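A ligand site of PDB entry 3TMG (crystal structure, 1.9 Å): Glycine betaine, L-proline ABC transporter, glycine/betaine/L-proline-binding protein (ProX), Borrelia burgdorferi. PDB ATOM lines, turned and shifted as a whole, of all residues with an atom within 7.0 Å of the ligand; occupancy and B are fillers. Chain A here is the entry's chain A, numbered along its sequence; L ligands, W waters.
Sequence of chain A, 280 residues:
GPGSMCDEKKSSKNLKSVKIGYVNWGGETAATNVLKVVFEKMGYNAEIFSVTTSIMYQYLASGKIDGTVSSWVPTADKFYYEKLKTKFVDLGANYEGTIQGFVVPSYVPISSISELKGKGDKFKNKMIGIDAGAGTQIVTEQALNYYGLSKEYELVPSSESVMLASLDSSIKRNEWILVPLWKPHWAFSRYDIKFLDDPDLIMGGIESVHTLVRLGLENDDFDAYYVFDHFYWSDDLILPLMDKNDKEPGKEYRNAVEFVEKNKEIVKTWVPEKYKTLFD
O1 of the ligand is in hydrogen-bond range of N of Thr 136. OG1 of Thr 136 lies within hydrogen-bond range of O2 of the ligand, 3.2 Å away. The backbone NH of Gly 135 lies within hydrogen-bond range of an oxygen (O1) of the ligand (3.4 Å).
OE1 of Gln 100 sits at hydrogen-bond distance from OG1 of Thr 136, 2.6 Å away. The side-chain carboxylate (OE2) of Glu 28 is in hydrogen-bond range of the indole nitrogen (NE1) of Trp 72, 2.9 Å away. The backbone NH of Asp 77 sits at hydrogen-bond distance from the backbone carbonyl oxygen of Trp 72 (2.9 Å). The backbone NH (N) of Ile 130 sits at hydrogen-bond distance from the side-chain amide oxygen (OE1) of Gln 137 (2.9 Å). The side-chain carboxylate of Asp 131 lies within hydrogen-bond range of the indole nitrogen of Trp 25 (3.0 Å).
Trp 25 touches the ligand. Glu 28 touches the ligand. Trp 72 touches the ligand (CG to O2, 3.3 Å). Ala 76 touches the ligand (CB to O2, 3.2 Å). Ile 130 touches the ligand (CD1 to C5, 3.6 Å). Trp 182 touches the ligand (CD2 to C4, 3.5 Å). Hydrophobic or aromatic side chains within 4 Å of the ligand: Trp 25, Trp 72, Ala 76, Ile 130 and Trp 182. Eight residues have an atom within 4 Å of the ligand: Trp 25, Glu 28, Trp 72, Ala 76, Ile 130, Gly 135, Thr 136 and Trp 182.
Water W1 lies within hydrogen-bond range of OD1 of Asp 77 (2.6 Å), O1 of the ligand (2.8 Å) and N of Gly 135 (2.9 Å). Water W2 lies within hydrogen-bond range of the side-chain carboxylate of Glu 28, the backbone NH of Gly 27 and the indole nitrogen of Trp 182.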
ATOM      1  N   TRP A  25       8.479 -13.494   1.200  1.00  0.00           N
ATOM      2  CA  TRP A  25       7.349 -14.240   1.784  1.00  0.00           C
ATOM      3  C   TRP A  25       7.955 -15.132   2.857  1.00  0.00           C
ATOM      4  O   TRP A  25       9.132 -15.517   2.749  1.00  0.00           O
ATOM      5  CB  TRP A  25       6.664 -15.135   0.767  1.00  0.00           C
ATOM      6  CG  TRP A  25       6.306 -14.417  -0.525  1.00  0.00           C
ATOM      7  CD1 TRP A  25       5.545 -13.281  -0.661  1.00  0.00           C
ATOM      8  CD2 TRP A  25       6.734 -14.760  -1.913  1.00  0.00           C
ATOM      9  NE1 TRP A  25       5.444 -12.903  -1.998  1.00  0.00           N
ATOM     10  CE2 TRP A  25       6.134 -13.757  -2.785  1.00  0.00           C
ATOM     11  CE3 TRP A  25       7.491 -15.776  -2.476  1.00  0.00           C
ATOM     12  CZ2 TRP A  25       6.311 -13.766  -4.164  1.00  0.00           C
ATOM     13  CZ3 TRP A  25       7.696 -15.790  -3.870  1.00  0.00           C
ATOM     14  CH2 TRP A  25       7.105 -14.801  -4.713  1.00  0.00           C
ATOM     15  N   GLY A  26       7.172 -15.496   3.853  1.00  0.00           N
ATOM     16  CA  GLY A  26       7.692 -16.339   4.940  1.00  0.00           C
ATOM     17  C   GLY A  26       8.421 -17.626   4.553  1.00  0.00           C
ATOM     18  O   GLY A  26       9.498 -17.895   5.088  1.00  0.00           O
ATOM     19  N   GLY A  27       7.851 -18.461   3.685  1.00  0.00           N
ATOM     20  CA  GLY A  27       8.501 -19.732   3.419  1.00  0.00           C
ATOM     21  C   GLY A  27       9.801 -19.506   2.603  1.00  0.00           C
ATOM     22  O   GLY A  27      10.848 -20.143   2.829  1.00  0.00           O
ATOM     23  N   GLU A  28       9.727 -18.618   1.627  1.00  0.00           N
ATOM     24  CA  GLU A  28      10.878 -18.381   0.765  1.00  0.00           C
ATOM     25  C   GLU A  28      12.038 -17.676   1.491  1.00  0.00           C
ATOM     26  O   GLU A  28      13.192 -17.954   1.239  1.00  0.00           O
ATOM     27  CB  GLU A  28      10.447 -17.563  -0.487  1.00  0.00           C
ATOM     28  CG  GLU A  28       9.719 -18.523  -1.464  1.00  0.00           C
ATOM     29  CD  GLU A  28       8.441 -19.213  -0.934  1.00  0.00           C
ATOM     30  OE1 GLU A  28       7.561 -18.494  -0.333  1.00  0.00           O
ATOM     31  OE2 GLU A  28       8.261 -20.479  -1.180  1.00  0.00           O
ATOM     32  N   THR A  53       9.242 -10.389  -7.430  1.00  0.00           N
ATOM     33  CA  THR A  53       9.166 -11.588  -8.270  1.00  0.00           C
ATOM     34  C   THR A  53       9.723 -11.363  -9.692  1.00  0.00           C
ATOM     35  O   THR A  53      10.493 -12.211 -10.192  1.00  0.00           O
ATOM     36  CB  THR A  53       7.717 -12.127  -8.328  1.00  0.00           C
ATOM     37  OG1 THR A  53       7.207 -12.222  -7.005  1.00  0.00           O
ATOM     38  CG2 THR A  53       7.693 -13.557  -8.919  1.00  0.00           C
ATOM     39  N   SER A  70      12.678 -20.271  -4.943  1.00  0.00           N
ATOM     40  CA  SER A  70      11.358 -19.638  -4.707  1.00  0.00           C
ATOM     41  C   SER A  70      10.366 -19.729  -5.868  1.00  0.00           C
ATOM     42  O   SER A  70       9.382 -19.010  -5.858  1.00  0.00           O
ATOM     43  CB  SER A  70      11.525 -18.164  -4.356  1.00  0.00           C
ATOM     44  OG  SER A  70      12.235 -18.015  -3.125  1.00  0.00           O
ATOM     45  N   SER A  71      10.589 -20.621  -6.843  1.00  0.00           N
ATOM     46  CA  SER A  71       9.705 -20.648  -8.031  1.00  0.00           C
ATOM     47  C   SER A  71       8.430 -21.474  -7.821  1.00  0.00           C
ATOM     48  O   SER A  71       8.512 -22.684  -7.582  1.00  0.00           O
ATOM     49  CB  SER A  71      10.481 -21.152  -9.268  1.00  0.00           C
ATOM     50  OG  SER A  71       9.658 -21.303 -10.424  1.00  0.00           O
ATOM     51  N   TRP A  72       7.270 -20.823  -7.910  1.00  0.00           N
ATOM     52  CA  TRP A  72       5.984 -21.525  -7.662  1.00  0.00           C
ATOM     53  C   TRP A  72       5.387 -21.879  -8.973  1.00  0.00           C
ATOM     54  O   TRP A  72       4.877 -21.009  -9.700  1.00  0.00           O
ATOM     55  CB  TRP A  72       5.014 -20.664  -6.859  1.00  0.00           C
ATOM     56  CG  TRP A  72       5.265 -20.761  -5.376  1.00  0.00           C
ATOM     57  CD1 TRP A  72       6.444 -20.457  -4.676  1.00  0.00           C
ATOM     58  CD2 TRP A  72       4.283 -21.105  -4.359  1.00  0.00           C
ATOM     59  NE1 TRP A  72       6.264 -20.688  -3.315  1.00  0.00           N
ATOM     60  CE2 TRP A  72       4.972 -21.079  -3.080  1.00  0.00           C
ATOM     61  CE3 TRP A  72       2.913 -21.457  -4.392  1.00  0.00           C
ATOM     62  CZ2 TRP A  72       4.314 -21.353  -1.886  1.00  0.00           C
ATOM     63  CZ3 TRP A  72       2.268 -21.749  -3.191  1.00  0.00           C
ATOM     64  CH2 TRP A  72       2.965 -21.696  -1.962  1.00  0.00           C
ATOM     65  N   VAL A  73       5.415 -23.175  -9.309  1.00  0.00           N
ATOM     66  CA  VAL A  73       5.055 -23.595 -10.682  1.00  0.00           C
ATOM     67  C   VAL A  73       4.252 -24.879 -10.695  1.00  0.00           C
ATOM     68  O   VAL A  73       4.385 -25.675  -9.745  1.00  0.00           O
ATOM     69  CB  VAL A  73       6.300 -23.858 -11.569  1.00  0.00           C
ATOM     70  CG1 VAL A  73       6.848 -22.531 -12.059  1.00  0.00           C
ATOM     71  CG2 VAL A  73       7.345 -24.655 -10.783  1.00  0.00           C
ATOM     72  N   THR A  75       1.549 -22.924 -11.927  1.00  0.00           N
ATOM     73  CA  THR A  75       0.458 -21.959 -12.052  1.00  0.00           C
ATOM     74  C   THR A  75       0.771 -20.546 -11.562  1.00  0.00           C
ATOM     75  O   THR A  75       0.591 -19.563 -12.326  1.00  0.00           O
ATOM     76  CB  THR A  75      -0.861 -22.436 -11.402  1.00  0.00           C
ATOM     77  OG1 THR A  75      -1.239 -23.672 -12.025  1.00  0.00           O
ATOM     78  CG2 THR A  75      -2.003 -21.357 -11.629  1.00  0.00           C
ATOM     79  N   ALA A  76       1.289 -20.451 -10.336  1.00  0.00           N
ATOM     80  CA  ALA A  76       1.478 -19.133  -9.718  1.00  0.00           C
ATOM     81  C   ALA A  76       2.395 -18.284 -10.562  1.00  0.00           C
ATOM     82  O   ALA A  76       2.079 -17.116 -10.833  1.00  0.00           O
ATOM     83  CB  ALA A  76       1.997 -19.256  -8.292  1.00  0.00           C
ATOM     84  N   ASP A  77       3.538 -18.841 -10.986  1.00  0.00           N
ATOM     85  CA  ASP A  77       4.534 -18.026 -11.676  1.00  0.00           C
ATOM     86  C   ASP A  77       4.540 -18.120 -13.194  1.00  0.00           C
ATOM     87  O   ASP A  77       5.511 -17.689 -13.817  1.00  0.00           O
ATOM     88  CB  ASP A  77       5.967 -18.311 -11.158  1.00  0.00           C
ATOM     89  CG  ASP A  77       6.173 -17.892  -9.716  1.00  0.00           C
ATOM     90  OD1 ASP A  77       5.227 -17.350  -9.050  1.00  0.00           O
ATOM     91  OD2 ASP A  77       7.289 -18.163  -9.232  1.00  0.00           O
ATOM     92  N   ILE A  99      -0.644 -25.238  -2.392  1.00  0.00           N
ATOM     93  CA  ILE A  99      -1.956 -24.897  -2.951  1.00  0.00           C
ATOM     94  C   ILE A  99      -2.059 -23.398  -2.783  1.00  0.00           C
ATOM     95  O   ILE A  99      -1.648 -22.865  -1.721  1.00  0.00           O
ATOM     96  CB  ILE A  99      -3.102 -25.575  -2.121  1.00  0.00           C
ATOM     97  CG1 ILE A  99      -3.020 -27.100  -2.152  1.00  0.00           C
ATOM     98  CG2 ILE A  99      -4.499 -25.039  -2.501  1.00  0.00           C
ATOM     99  CD1 ILE A  99      -4.033 -27.787  -1.220  1.00  0.00           C
ATOM    100  N   GLN A 100      -2.625 -22.696  -3.764  1.00  0.00           N
ATOM    101  CA  GLN A 100      -2.968 -21.279  -3.571  1.00  0.00           C
ATOM    102  C   GLN A 100      -4.456 -21.157  -3.868  1.00  0.00           C
ATOM    103  O   GLN A 100      -5.019 -21.966  -4.616  1.00  0.00           O
ATOM    104  CB  GLN A 100      -2.125 -20.360  -4.501  1.00  0.00           C
ATOM    105  CG  GLN A 100      -2.174 -20.787  -5.975  1.00  0.00           C
ATOM    106  CD  GLN A 100      -1.715 -19.739  -6.983  1.00  0.00           C
ATOM    107  OE1 GLN A 100      -1.060 -18.742  -6.635  1.00  0.00           O
ATOM    108  NE2 GLN A 100      -2.026 -19.987  -8.279  1.00  0.00           N
ATOM    109  N   ILE A 130      -1.806  -9.535  -1.534  1.00  0.00           N
ATOM    110  CA  ILE A 130      -0.402  -9.419  -1.110  1.00  0.00           C
ATOM    111  C   ILE A 130       0.342  -8.471  -2.094  1.00  0.00           C
ATOM    112  O   ILE A 130      -0.304  -7.585  -2.676  1.00  0.00           O
ATOM    113  CB  ILE A 130       0.276 -10.806  -0.954  1.00  0.00           C
ATOM    114  CG1 ILE A 130       0.276 -11.584  -2.288  1.00  0.00           C
ATOM    115  CG2 ILE A 130      -0.418 -11.650   0.131  1.00  0.00           C
ATOM    116  CD1 ILE A 130       1.144 -12.845  -2.278  1.00  0.00           C
ATOM    117  N   ASP A 131       1.666  -8.619  -2.244  1.00  0.00           N
ATOM    118  CA  ASP A 131       2.465  -7.751  -3.099  1.00  0.00           C
ATOM    119  C   ASP A 131       2.009  -7.746  -4.564  1.00  0.00           C
ATOM    120  O   ASP A 131       1.796  -8.831  -5.157  1.00  0.00           O
ATOM    121  CB  ASP A 131       3.997  -8.009  -2.947  1.00  0.00           C
ATOM    122  CG  ASP A 131       4.394  -9.537  -2.967  1.00  0.00           C
ATOM    123  OD1 ASP A 131       3.857 -10.326  -2.188  1.00  0.00           O
ATOM    124  OD2 ASP A 131       5.291  -9.933  -3.752  1.00  0.00           O
ATOM    125  N   GLY A 133       2.250  -8.035  -8.327  1.00  0.00           N
ATOM    126  CA  GLY A 133       3.237  -8.734  -9.131  1.00  0.00           C
ATOM    127  C   GLY A 133       3.614 -10.116  -8.625  1.00  0.00           C
ATOM    128  O   GLY A 133       4.204 -10.890  -9.370  1.00  0.00           O
ATOM    129  N   ALA A 134       3.249 -10.459  -7.388  1.00  0.00           N
ATOM    130  CA  ALA A 134       3.448 -11.812  -6.906  1.00  0.00           C
ATOM    131  C   ALA A 134       2.638 -12.744  -7.797  1.00  0.00           C
ATOM    132  O   ALA A 134       1.545 -12.402  -8.215  1.00  0.00           O
ATOM    133  CB  ALA A 134       2.977 -11.955  -5.427  1.00  0.00           C
ATOM    134  N   GLY A 135       3.151 -13.939  -8.076  1.00  0.00           N
ATOM    135  CA  GLY A 135       2.407 -14.870  -8.912  1.00  0.00           C
ATOM    136  C   GLY A 135       0.991 -15.083  -8.383  1.00  0.00           C
ATOM    137  O   GLY A 135       0.007 -14.993  -9.127  1.00  0.00           O
ATOM    138  N   THR A 136       0.893 -15.340  -7.080  1.00  0.00           N
ATOM    139  CA  THR A 136      -0.420 -15.572  -6.497  1.00  0.00           C
ATOM    140  C   THR A 136      -1.366 -14.360  -6.701  1.00  0.00           C
ATOM    141  O   THR A 136      -2.562 -14.512  -6.946  1.00  0.00           O
ATOM    142  CB  THR A 136      -0.319 -15.953  -5.019  1.00  0.00           C
ATOM    143  OG1 THR A 136       0.262 -17.267  -4.926  1.00  0.00           O
ATOM    144  CG2 THR A 136      -1.729 -16.026  -4.389  1.00  0.00           C
ATOM    145  N   GLN A 137      -0.818 -13.158  -6.591  1.00  0.00           N
ATOM    146  CA  GLN A 137      -1.624 -11.956  -6.828  1.00  0.00           C
ATOM    147  C   GLN A 137      -2.111 -11.818  -8.276  1.00  0.00           C
ATOM    148  O   GLN A 137      -3.261 -11.436  -8.552  1.00  0.00           O
ATOM    149  CB  GLN A 137      -0.815 -10.711  -6.452  1.00  0.00           C
ATOM    150  CG  GLN A 137      -1.597  -9.382  -6.440  1.00  0.00           C
ATOM    151  CD  GLN A 137      -2.393  -9.161  -5.156  1.00  0.00           C
ATOM    152  OE1 GLN A 137      -2.498 -10.049  -4.315  1.00  0.00           O
ATOM    153  NE2 GLN A 137      -3.033  -7.986  -5.056  1.00  0.00           N
ATOM    154  N   GLU A 160       2.286  -9.748   2.279  1.00  0.00           N
ATOM    155  CA  GLU A 160       1.946 -10.884   3.123  1.00  0.00           C
ATOM    156  C   GLU A 160       1.652 -10.404   4.579  1.00  0.00           C
ATOM    157  O   GLU A 160       0.687 -10.853   5.160  1.00  0.00           O
ATOM    158  CB  GLU A 160       3.028 -11.965   3.133  1.00  0.00           C
ATOM    159  CG  GLU A 160       2.577 -13.240   3.873  1.00  0.00           C
ATOM    160  CD  GLU A 160       3.674 -14.268   4.164  1.00  0.00           C
ATOM    161  OE1 GLU A 160       4.831 -14.016   3.790  1.00  0.00           O
ATOM    162  OE2 GLU A 160       3.411 -15.333   4.783  1.00  0.00           O
ATOM    163  N   LEU A 181      -4.587 -16.904  -0.025  1.00  0.00           N
ATOM    164  CA  LEU A 181      -3.636 -17.537   0.905  1.00  0.00           C
ATOM    165  C   LEU A 181      -3.150 -18.820   0.241  1.00  0.00           C
ATOM    166  O   LEU A 181      -3.524 -19.138  -0.888  1.00  0.00           O
ATOM    167  CB  LEU A 181      -4.230 -17.799   2.301  1.00  0.00           C
ATOM    168  CG  LEU A 181      -3.589 -16.956   3.407  1.00  0.00           C
ATOM    169  CD1 LEU A 181      -4.322 -17.088   4.732  1.00  0.00           C
ATOM    170  CD2 LEU A 181      -2.104 -17.300   3.592  1.00  0.00           C
ATOM    171  N   TRP A 182      -2.268 -19.544   0.922  1.00  0.00           N
ATOM    172  CA  TRP A 182      -1.625 -20.661   0.289  1.00  0.00           C
ATOM    173  C   TRP A 182      -1.167 -21.573   1.374  1.00  0.00           C
ATOM    174  O   TRP A 182      -1.121 -21.160   2.574  1.00  0.00           O
ATOM    175  CB  TRP A 182      -0.429 -20.199  -0.597  1.00  0.00           C
ATOM    176  CG  TRP A 182       0.584 -19.364   0.178  1.00  0.00           C
ATOM    177  CD1 TRP A 182       1.687 -19.794   0.932  1.00  0.00           C
ATOM    178  CD2 TRP A 182       0.533 -17.917   0.332  1.00  0.00           C
ATOM    179  NE1 TRP A 182       2.346 -18.706   1.488  1.00  0.00           N
ATOM    180  CE2 TRP A 182       1.675 -17.550   1.179  1.00  0.00           C
ATOM    181  CE3 TRP A 182      -0.314 -16.915  -0.171  1.00  0.00           C
ATOM    182  CZ2 TRP A 182       1.945 -16.226   1.511  1.00  0.00           C
ATOM    183  CZ3 TRP A 182      -0.050 -15.586   0.183  1.00  0.00           C
ATOM    184  CH2 TRP A 182       1.064 -15.241   0.989  1.00  0.00           C
ATOM    185  N   LYS A 183      -0.874 -22.813   0.977  1.00  0.00           N
ATOM    186  CA  LYS A 183      -0.144 -23.728   1.841  1.00  0.00           C
ATOM    187  C   LYS A 183       1.165 -24.040   1.132  1.00  0.00           C
ATOM    188  O   LYS A 183       1.210 -24.127  -0.105  1.00  0.00           O
ATOM    189  CB  LYS A 183      -0.945 -25.042   2.127  1.00  0.00           C
ATOM    190  CG  LYS A 183      -2.231 -24.821   2.889  1.00  0.00           C
ATOM    191  CD  LYS A 183      -2.966 -26.148   3.167  1.00  0.00           C
ATOM    192  CE  LYS A 183      -4.024 -25.988   4.264  1.00  0.00           C
ATOM    193  NZ  LYS A 183      -4.940 -27.184   4.279  1.00  0.00           N
ATOM    194  N   PRO A 184       2.243 -24.237   1.912  1.00  0.00           N
ATOM    195  CA  PRO A 184       2.309 -24.348   3.359  1.00  0.00           C
ATOM    196  C   PRO A 184       2.240 -22.985   4.049  1.00  0.00           C
ATOM    197  O   PRO A 184       2.937 -22.058   3.626  1.00  0.00           O
ATOM    198  CB  PRO A 184       3.690 -24.997   3.618  1.00  0.00           C
ATOM    199  CG  PRO A 184       4.520 -24.532   2.424  1.00  0.00           C
ATOM    200  CD  PRO A 184       3.534 -24.466   1.257  1.00  0.00           C
ATOM    201  N   HIS A 185       1.430 -22.874   5.097  1.00  0.00           N
ATOM    202  CA  HIS A 185       1.406 -21.634   5.875  1.00  0.00           C
ATOM    203  C   HIS A 185       0.875 -21.957   7.244  1.00  0.00           C
ATOM    204  O   HIS A 185      -0.099 -22.736   7.371  1.00  0.00           O
ATOM    205  CB  HIS A 185       0.564 -20.532   5.184  1.00  0.00           C
ATOM    206  CG  HIS A 185       0.929 -19.127   5.623  1.00  0.00           C
ATOM    207  ND1 HIS A 185       0.622 -18.666   6.853  1.00  0.00           N
ATOM    208  CD2 HIS A 185       1.656 -18.114   4.998  1.00  0.00           C
ATOM    209  CE1 HIS A 185       1.058 -17.376   6.991  1.00  0.00           C
ATOM    210  NE2 HIS A 185       1.689 -17.038   5.866  1.00  0.00           N
HETATM  211  N1  LIG L   1       3.560 -17.241  -2.578  1.00  0.00           N
HETATM  212  C1  LIG L   1       4.435 -17.407  -3.753  1.00  0.00           C
HETATM  213  C2  LIG L   1       3.604 -17.135  -5.012  1.00  0.00           C
HETATM  214  O1  LIG L   1       3.267 -15.987  -5.417  1.00  0.00           O
HETATM  215  O2  LIG L   1       3.231 -18.131  -5.589  1.00  0.00           O
HETATM  216  C3  LIG L   1       4.240 -17.624  -1.330  1.00  0.00           C
HETATM  217  C4  LIG L   1       2.367 -18.074  -2.702  1.00  0.00           C
HETATM  218  C5  LIG L   1       3.132 -15.829  -2.495  1.00  0.00           C
HETATM  219  O   HOH W   1       5.416 -15.543  -7.141  1.00  0.00           O
HETATM  220  O   HOH W   2       5.748 -18.611   1.359  1.00  0.00           O
